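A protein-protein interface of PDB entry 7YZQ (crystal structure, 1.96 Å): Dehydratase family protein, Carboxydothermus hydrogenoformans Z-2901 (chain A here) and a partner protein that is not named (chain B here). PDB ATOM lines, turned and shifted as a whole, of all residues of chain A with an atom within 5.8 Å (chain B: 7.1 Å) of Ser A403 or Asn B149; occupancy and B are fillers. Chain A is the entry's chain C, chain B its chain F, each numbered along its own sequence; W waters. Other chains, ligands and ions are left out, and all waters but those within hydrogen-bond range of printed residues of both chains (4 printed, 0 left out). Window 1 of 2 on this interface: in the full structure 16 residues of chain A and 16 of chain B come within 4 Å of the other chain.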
ATOM      1  N   GLN A  99      16.140  19.891  -5.474  1.00  0.00           N
ATOM      2  CA  GLN A  99      14.784  20.417  -5.496  1.00  0.00           C
ATOM      3  C   GLN A  99      14.287  20.611  -6.923  1.00  0.00           C
ATOM      4  O   GLN A  99      13.069  20.555  -7.178  1.00  0.00           O
ATOM      5  CB  GLN A  99      14.718  21.739  -4.731  1.00  0.00           C
ATOM      6  CG  GLN A  99      13.320  22.384  -4.745  1.00  0.00           C
ATOM      7  CD  GLN A  99      12.274  21.678  -3.923  1.00  0.00           C
ATOM      8  OE1 GLN A  99      12.588  20.992  -2.952  1.00  0.00           O
ATOM      9  NE2 GLN A  99      10.996  21.814  -4.337  1.00  0.00           N
ATOM     10  N   LYS A 291      23.187  21.510   2.635  1.00  0.00           N
ATOM     11  CA  LYS A 291      22.721  22.692   3.373  1.00  0.00           C
ATOM     12  C   LYS A 291      23.003  22.609   4.881  1.00  0.00           C
ATOM     13  O   LYS A 291      23.493  23.578   5.504  1.00  0.00           O
ATOM     14  CB  LYS A 291      21.218  22.862   3.107  1.00  0.00           C
ATOM     15  CG  LYS A 291      20.495  23.874   4.002  1.00  0.00           C
ATOM     16  CD  LYS A 291      19.069  24.132   3.433  1.00  0.00           C
ATOM     17  CE  LYS A 291      18.112  22.990   3.739  1.00  0.00           C
ATOM     18  NZ  LYS A 291      16.740  23.121   3.110  1.00  0.00           N
ATOM     19  N   SER A 400      13.913  19.467   7.102  1.00  0.00           N
ATOM     20  CA  SER A 400      13.792  20.361   5.964  1.00  0.00           C
ATOM     21  C   SER A 400      13.554  19.508   4.715  1.00  0.00           C
ATOM     22  O   SER A 400      13.459  18.273   4.771  1.00  0.00           O
ATOM     23  CB  SER A 400      15.048  21.236   5.852  1.00  0.00           C
ATOM     24  OG  SER A 400      14.868  22.164   4.852  1.00  0.00           O
ATOM     25  N   ASP A 401      13.488  20.176   3.583  1.00  0.00           N
ATOM     26  CA  ASP A 401      13.442  19.533   2.287  1.00  0.00           C
ATOM     27  C   ASP A 401      14.578  20.109   1.462  1.00  0.00           C
ATOM     28  O   ASP A 401      15.509  20.694   1.997  1.00  0.00           O
ATOM     29  CB  ASP A 401      12.053  19.664   1.649  1.00  0.00           C
ATOM     30  CG  ASP A 401      11.604  21.093   1.448  1.00  0.00           C
ATOM     31  OD1 ASP A 401      12.439  21.944   1.101  1.00  0.00           O
ATOM     32  OD2 ASP A 401      10.386  21.343   1.596  1.00  0.00           O
ATOM     33  N   PHE A 402      14.564  19.834   0.166  1.00  0.00           N
ATOM     34  CA  PHE A 402      15.704  20.192  -0.669  1.00  0.00           C
ATOM     35  C   PHE A 402      15.676  21.655  -1.098  1.00  0.00           C
ATOM     36  O   PHE A 402      16.677  22.179  -1.603  1.00  0.00           O
ATOM     37  CB  PHE A 402      15.749  19.250  -1.898  1.00  0.00           C
ATOM     38  CG  PHE A 402      16.012  17.827  -1.563  1.00  0.00           C
ATOM     39  CD1 PHE A 402      16.636  17.477  -0.383  1.00  0.00           C
ATOM     40  CD2 PHE A 402      15.628  16.806  -2.444  1.00  0.00           C
ATOM     41  CE1 PHE A 402      16.848  16.143  -0.091  1.00  0.00           C
ATOM     42  CE2 PHE A 402      15.872  15.504  -2.148  1.00  0.00           C
ATOM     43  CZ  PHE A 402      16.506  15.170  -0.978  1.00  0.00           C
ATOM     44  N   SER A 403      14.556  22.330  -0.911  1.00  0.00           N
ATOM     45  CA  SER A 403      14.491  23.753  -1.200  1.00  0.00           C
ATOM     46  C   SER A 403      15.511  24.482  -0.343  1.00  0.00           C
ATOM     47  O   SER A 403      15.540  24.332   0.876  1.00  0.00           O
ATOM     48  CB  SER A 403      13.071  24.257  -0.958  1.00  0.00           C
ATOM     49  OG  SER A 403      12.932  25.568  -1.425  1.00  0.00           O
ATOM     50  N   GLU A 404      16.357  25.266  -0.980  1.00  0.00           N
ATOM     51  CA  GLU A 404      17.546  25.781  -0.312  1.00  0.00           C
ATOM     52  C   GLU A 404      17.330  27.055   0.507  1.00  0.00           C
ATOM     53  O   GLU A 404      18.238  27.472   1.235  1.00  0.00           O
ATOM     54  CB  GLU A 404      18.642  26.096  -1.337  1.00  0.00           C
ATOM     55  CG  GLU A 404      19.212  24.852  -2.003  1.00  0.00           C
ATOM     56  CD  GLU A 404      20.385  25.151  -2.908  1.00  0.00           C
ATOM     57  OE1 GLU A 404      21.539  25.150  -2.416  1.00  0.00           O
ATOM     58  OE2 GLU A 404      20.163  25.388  -4.118  1.00  0.00           O
ATOM     59  N   GLU A 405      16.171  27.672   0.447  1.00  0.00           N
ATOM     60  CA  GLU A 405      16.017  29.053   0.908  1.00  0.00           C
ATOM     61  C   GLU A 405      15.394  29.195   2.301  1.00  0.00           C
ATOM     62  O   GLU A 405      15.074  30.324   2.728  1.00  0.00           O
ATOM     63  CB  GLU A 405      15.197  29.836  -0.116  1.00  0.00           C
ATOM     64  CG  GLU A 405      15.920  29.994  -1.488  1.00  0.00           C
ATOM     65  CD  GLU A 405      17.399  30.415  -1.375  1.00  0.00           C
ATOM     66  OE1 GLU A 405      18.165  30.099  -2.299  1.00  0.00           O
ATOM     67  OE2 GLU A 405      17.808  31.065  -0.379  1.00  0.00           O
ATOM     68  N   ASP A 406      15.230  28.098   3.034  1.00  0.00           N
ATOM     69  CA  ASP A 406      14.789  28.184   4.423  1.00  0.00           C
ATOM     70  C   ASP A 406      16.006  28.339   5.315  1.00  0.00           C
ATOM     71  O   ASP A 406      15.998  27.922   6.480  1.00  0.00           O
ATOM     72  CB  ASP A 406      13.965  26.966   4.844  1.00  0.00           C
ATOM     73  CG  ASP A 406      14.766  25.628   4.778  1.00  0.00           C
ATOM     74  OD1 ASP A 406      15.762  25.523   3.998  1.00  0.00           O
ATOM     75  OD2 ASP A 406      14.356  24.709   5.537  1.00  0.00           O
ATOM     76  N   PHE B 122      -2.144  34.191  -1.346  1.00  0.00           N
ATOM     77  CA  PHE B 122      -0.781  34.429  -0.893  1.00  0.00           C
ATOM     78  C   PHE B 122      -0.059  35.383  -1.824  1.00  0.00           C
ATOM     79  O   PHE B 122       0.678  36.268  -1.365  1.00  0.00           O
ATOM     80  CB  PHE B 122      -0.023  33.101  -0.808  1.00  0.00           C
ATOM     81  CG  PHE B 122       1.440  33.236  -0.498  1.00  0.00           C
ATOM     82  CD1 PHE B 122       1.836  33.748   0.687  1.00  0.00           C
ATOM     83  CD2 PHE B 122       2.406  32.788  -1.387  1.00  0.00           C
ATOM     84  CE1 PHE B 122       3.205  33.841   0.999  1.00  0.00           C
ATOM     85  CE2 PHE B 122       3.743  32.883  -1.106  1.00  0.00           C
ATOM     86  CZ  PHE B 122       4.146  33.393   0.109  1.00  0.00           C
ATOM     87  N   VAL B 146      14.828  33.549  -7.963  1.00  0.00           N
ATOM     88  CA  VAL B 146      15.252  32.612  -6.929  1.00  0.00           C
ATOM     89  C   VAL B 146      14.138  31.588  -6.772  1.00  0.00           C
ATOM     90  O   VAL B 146      13.006  31.983  -6.443  1.00  0.00           O
ATOM     91  CB  VAL B 146      15.552  33.332  -5.607  1.00  0.00           C
ATOM     92  CG1 VAL B 146      16.716  34.322  -5.818  1.00  0.00           C
ATOM     93  CG2 VAL B 146      14.337  34.100  -5.094  1.00  0.00           C
ATOM     94  N   PRO B 147      14.393  30.295  -7.030  1.00  0.00           N
ATOM     95  CA  PRO B 147      13.336  29.279  -6.871  1.00  0.00           C
ATOM     96  C   PRO B 147      12.858  29.213  -5.425  1.00  0.00           C
ATOM     97  O   PRO B 147      13.652  29.140  -4.483  1.00  0.00           O
ATOM     98  CB  PRO B 147      14.000  27.962  -7.325  1.00  0.00           C
ATOM     99  CG  PRO B 147      15.496  28.252  -7.416  1.00  0.00           C
ATOM    100  CD  PRO B 147      15.664  29.742  -7.551  1.00  0.00           C
ATOM    101  N   ILE B 148      11.547  29.225  -5.266  1.00  0.00           N
ATOM    102  CA  ILE B 148      10.901  29.247  -3.967  1.00  0.00           C
ATOM    103  C   ILE B 148      10.156  27.938  -3.816  1.00  0.00           C
ATOM    104  O   ILE B 148       9.688  27.352  -4.793  1.00  0.00           O
ATOM    105  CB  ILE B 148      10.000  30.497  -3.802  1.00  0.00           C
ATOM    106  CG1 ILE B 148      10.953  31.727  -3.792  1.00  0.00           C
ATOM    107  CG2 ILE B 148       9.171  30.407  -2.551  1.00  0.00           C
ATOM    108  CD1 ILE B 148      10.382  32.984  -3.274  1.00  0.00           C
ATOM    109  N   ASN B 149      10.104  27.447  -2.586  1.00  0.00           N
ATOM    110  CA  ASN B 149       9.502  26.141  -2.333  1.00  0.00           C
ATOM    111  C   ASN B 149       8.087  26.104  -2.884  1.00  0.00           C
ATOM    112  O   ASN B 149       7.320  27.057  -2.733  1.00  0.00           O
ATOM    113  CB  ASN B 149       9.495  25.845  -0.825  1.00  0.00           C
ATOM    114  CG  ASN B 149       9.423  24.375  -0.512  1.00  0.00           C
ATOM    115  OD1 ASN B 149       8.707  23.629  -1.167  1.00  0.00           O
ATOM    116  ND2 ASN B 149      10.172  23.946   0.507  1.00  0.00           N
ATOM    117  N   SER B 150       7.744  24.998  -3.531  1.00  0.00           N
ATOM    118  CA  SER B 150       6.434  24.831  -4.148  1.00  0.00           C
ATOM    119  C   SER B 150       5.496  23.993  -3.288  1.00  0.00           C
ATOM    120  O   SER B 150       4.347  23.779  -3.675  1.00  0.00           O
ATOM    121  CB  SER B 150       6.585  24.183  -5.544  1.00  0.00           C
ATOM    122  OG  SER B 150       7.389  22.993  -5.511  1.00  0.00           O
ATOM    123  N   MET B 151       5.951  23.529  -2.125  1.00  0.00           N
ATOM    124  CA  MET B 151       5.106  22.707  -1.272  1.00  0.00           C
ATOM    125  C   MET B 151       3.782  23.393  -0.936  1.00  0.00           C
ATOM    126  O   MET B 151       2.710  22.799  -1.097  1.00  0.00           O
ATOM    127  CB  MET B 151       5.856  22.357   0.012  1.00  0.00           C
ATOM    128  CG  MET B 151       5.096  21.497   0.948  1.00  0.00           C
ATOM    129  SD  MET B 151       4.969  19.802   0.259  1.00  0.00           S
ATOM    130  CE  MET B 151       6.520  19.078   0.646  1.00  0.00           C
ATOM    131  N   CYS B 152       3.841  24.600  -0.382  1.00  0.00           N
ATOM    132  CA  CYS B 152       2.664  25.275   0.146  1.00  0.00           C
ATOM    133  C   CYS B 152       3.079  26.698   0.441  1.00  0.00           C
ATOM    134  O   CYS B 152       4.266  27.044   0.396  1.00  0.00           O
ATOM    135  CB  CYS B 152       2.151  24.569   1.400  1.00  0.00           C
ATOM    136  SG  CYS B 152       3.399  24.671   2.726  1.00  0.00           S
ATOM    137  N   THR B 153       2.087  27.509   0.785  1.00  0.00           N
ATOM    138  CA  THR B 153       2.345  28.914   1.051  1.00  0.00           C
ATOM    139  C   THR B 153       3.008  29.146   2.414  1.00  0.00           C
ATOM    140  O   THR B 153       3.638  30.192   2.593  1.00  0.00           O
ATOM    141  CB  THR B 153       1.059  29.766   0.981  1.00  0.00           C
ATOM    142  OG1 THR B 153       0.168  29.346   1.997  1.00  0.00           O
ATOM    143  CG2 THR B 153       0.399  29.659  -0.357  1.00  0.00           C
ATOM    144  N   PHE B 155       5.564  27.186   3.669  1.00  0.00           N
ATOM    145  CA  PHE B 155       6.993  27.027   3.390  1.00  0.00           C
ATOM    146  C   PHE B 155       7.504  28.151   2.483  1.00  0.00           C
ATOM    147  O   PHE B 155       8.669  28.554   2.572  1.00  0.00           O
ATOM    148  CB  PHE B 155       7.269  25.678   2.716  1.00  0.00           C
ATOM    149  CG  PHE B 155       7.075  24.459   3.586  1.00  0.00           C
ATOM    150  CD1 PHE B 155       6.294  24.490   4.698  1.00  0.00           C
ATOM    151  CD2 PHE B 155       7.701  23.261   3.244  1.00  0.00           C
ATOM    152  CE1 PHE B 155       6.102  23.346   5.490  1.00  0.00           C
ATOM    153  CE2 PHE B 155       7.538  22.123   3.992  1.00  0.00           C
ATOM    154  CZ  PHE B 155       6.720  22.157   5.137  1.00  0.00           C
ATOM    155  N   ALA B 156       6.654  28.638   1.573  1.00  0.00           N
ATOM    156  CA  ALA B 156       7.069  29.707   0.682  1.00  0.00           C
ATOM    157  C   ALA B 156       7.257  31.011   1.455  1.00  0.00           C
ATOM    158  O   ALA B 156       8.222  31.732   1.219  1.00  0.00           O
ATOM    159  CB  ALA B 156       6.059  29.886  -0.455  1.00  0.00           C
ATOM    160  N   GLU B 157       6.345  31.326   2.375  1.00  0.00           N
ATOM    161  CA  GLU B 157       6.494  32.511   3.222  1.00  0.00           C
ATOM    162  C   GLU B 157       7.790  32.438   4.027  1.00  0.00           C
ATOM    163  O   GLU B 157       8.548  33.410   4.097  1.00  0.00           O
ATOM    164  CB  GLU B 157       5.287  32.645   4.153  1.00  0.00           C
ATOM    165  CG  GLU B 157       5.321  33.912   4.980  1.00  0.00           C
ATOM    166  CD  GLU B 157       4.180  33.997   5.993  1.00  0.00           C
ATOM    167  OE1 GLU B 157       3.833  35.128   6.388  1.00  0.00           O
ATOM    168  OE2 GLU B 157       3.640  32.941   6.408  1.00  0.00           O
ATOM    169  N   GLU B 159      10.509  31.089   3.274  1.00  0.00           N
ATOM    170  CA  GLU B 159      11.672  31.346   2.423  1.00  0.00           C
ATOM    171  C   GLU B 159      11.723  32.800   2.003  1.00  0.00           C
ATOM    172  O   GLU B 159      12.803  33.403   1.936  1.00  0.00           O
ATOM    173  CB  GLU B 159      11.656  30.448   1.180  1.00  0.00           C
ATOM    174  CG  GLU B 159      12.011  29.033   1.468  1.00  0.00           C
ATOM    175  CD  GLU B 159      12.117  28.189   0.235  1.00  0.00           C
ATOM    176  OE1 GLU B 159      11.670  28.624  -0.851  1.00  0.00           O
ATOM    177  OE2 GLU B 159      12.699  27.106   0.349  1.00  0.00           O
ATOM    178  N   LEU B 177       8.739  33.802  -7.143  1.00  0.00           N
ATOM    179  CA  LEU B 177       7.433  33.299  -6.728  1.00  0.00           C
ATOM    180  C   LEU B 177       6.531  32.999  -7.926  1.00  0.00           C
ATOM    181  O   LEU B 177       5.856  31.970  -7.958  1.00  0.00           O
ATOM    182  CB  LEU B 177       6.750  34.301  -5.808  1.00  0.00           C
ATOM    183  CG  LEU B 177       7.247  34.305  -4.364  1.00  0.00           C
ATOM    184  CD1 LEU B 177       6.424  35.300  -3.598  1.00  0.00           C
ATOM    185  CD2 LEU B 177       7.156  32.911  -3.725  1.00  0.00           C
ATOM    186  N   THR B 180       7.970  29.881  -9.859  1.00  0.00           N
ATOM    187  CA  THR B 180       7.647  28.644  -9.154  1.00  0.00           C
ATOM    188  C   THR B 180       6.150  28.365  -9.208  1.00  0.00           C
ATOM    189  O   THR B 180       5.726  27.208  -9.303  1.00  0.00           O
ATOM    190  CB  THR B 180       8.131  28.726  -7.693  1.00  0.00           C
ATOM    191  OG1 THR B 180       9.557  28.855  -7.672  1.00  0.00           O
ATOM    192  CG2 THR B 180       7.747  27.486  -6.889  1.00  0.00           C
ATOM    193  N   THR B 181       5.329  29.397  -9.061  1.00  0.00           N
ATOM    194  CA  THR B 181       3.888  29.191  -9.165  1.00  0.00           C
ATOM    195  C   THR B 181       3.510  28.737 -10.582  1.00  0.00           C
ATOM    196  O   THR B 181       2.629  27.886 -10.763  1.00  0.00           O
ATOM    197  CB  THR B 181       3.150  30.477  -8.755  1.00  0.00           C
ATOM    198  OG1 THR B 181       3.412  30.767  -7.371  1.00  0.00           O
ATOM    199  CG2 THR B 181       1.617  30.352  -8.901  1.00  0.00           C
ATOM    200  N   ARG B 184       4.545  24.914 -10.982  1.00  0.00           N
ATOM    201  CA  ARG B 184       3.632  23.960 -10.350  1.00  0.00           C
ATOM    202  C   ARG B 184       2.275  23.914 -11.073  1.00  0.00           C
ATOM    203  O   ARG B 184       1.676  22.845 -11.262  1.00  0.00           O
ATOM    204  CB  ARG B 184       3.439  24.310  -8.870  1.00  0.00           C
ATOM    205  CG  ARG B 184       2.855  23.137  -8.062  1.00  0.00           C
ATOM    206  CD  ARG B 184       2.510  23.488  -6.599  1.00  0.00           C
ATOM    207  NE  ARG B 184       1.871  24.797  -6.420  1.00  0.00           N
ATOM    208  CZ  ARG B 184       2.546  25.930  -6.197  1.00  0.00           C
ATOM    209  NH1 ARG B 184       1.908  27.088  -6.027  1.00  0.00           N
ATOM    210  NH2 ARG B 184       3.878  25.913  -6.114  1.00  0.00           N
HETATM  211  O   HOH W   1       8.860  21.084  -2.380  1.00  0.00           O
HETATM  212  O   HOH W   2       9.892  23.553  -6.124  1.00  0.00           O
HETATM  213  O   HOH W   3      16.709  28.712  -4.405  1.00  0.00           O
HETATM  214  O   HOH W   4      13.426  26.200  -3.995  1.00  0.00           O
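Printed residues of chain A that touch a printed residue of chain B: Gln A99, Asp A401, Ser A403, Glu A405 and Asp A406. Of the 17 printed residues of chain B, 5 touch a printed residue of chain A. Printed residues of chain B that touch a printed residue of chain A: Pro B147, Asn B149, Ser B150, Phe B155 and Glu B159. Hydrophobic or aromatic side chains of chain B within 4 Å of the printed part of chain A: Phe B155.
Among the printed residues, pairs that only touch across the chains: Ser A403 with Asn B149, Glu A405 with Glu B159, Asp A401 with Phe B155, Asp A406 with Glu B159, Glu A405 with Pro B147 and Gln A99 with Ser B150.
Printed residues of chain B within 4 Å of Gln A99: Ser B150. Of the printed residues of chain B, Asp A401 touches Asn B149 (2.8 Å) and Phe B155 (3.7 Å). Of chain B, only Asn B149 and Glu B159 come within 4 Å of Ser A403. Printed residues of chain A within 4 Å of Pro B147: Glu A405 (3.9 Å). Asn B149 touches two residues of chain A. Of the printed residues of chain A, Phe B155 touches Asp A401 (3.7 Å). Arg B184 touches none of the printed residues of chain A.
Water W2 lies within hydrogen-bond range of the side-chain hydroxyl of Ser B150 and the side-chain amide nitrogen of Gln A99. Water W4 lies within hydrogen-bond range of OG of Ser A403 and O of Pro B147. Water W1 bridges the side-chain amide oxygen of Asn B149 (2.8 Å) and the side-chain amide nitrogen of Gln A99 (3.0 Å). Water W3 lies within hydrogen-bond range of OE1 of Glu A405 and O of Pro B147.
N of Ser A403 is in hydrogen-bond range of OE1 of Gln A99. The side-chain sulfur of Cys B152 sits close to the backbone NH of Phe B155. The side-chain carboxylate of Asp A406 is in salt-bridge range of the side-chain amino group of Lys A291 (2.7 Å). The backbone carbonyl oxygen of Asp A401 sits at hydrogen-bond distance from the side-chain amino group of Lys A291 (2.9 Å). NZ of Lys A291 sits at hydrogen-bond distance from O of Ser A403 (2.8 Å). OE1 of Glu B159 is in hydrogen-bond range of N of Asn B149 (2.6 Å).
The side-chain carboxylate (OD2) of Asp A401 is in hydrogen-bond range of the side-chain amide nitrogen (ND2) of Asn B149. OE1 of Glu B159 sits close to OG of Ser A403, 3.4 Å away.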
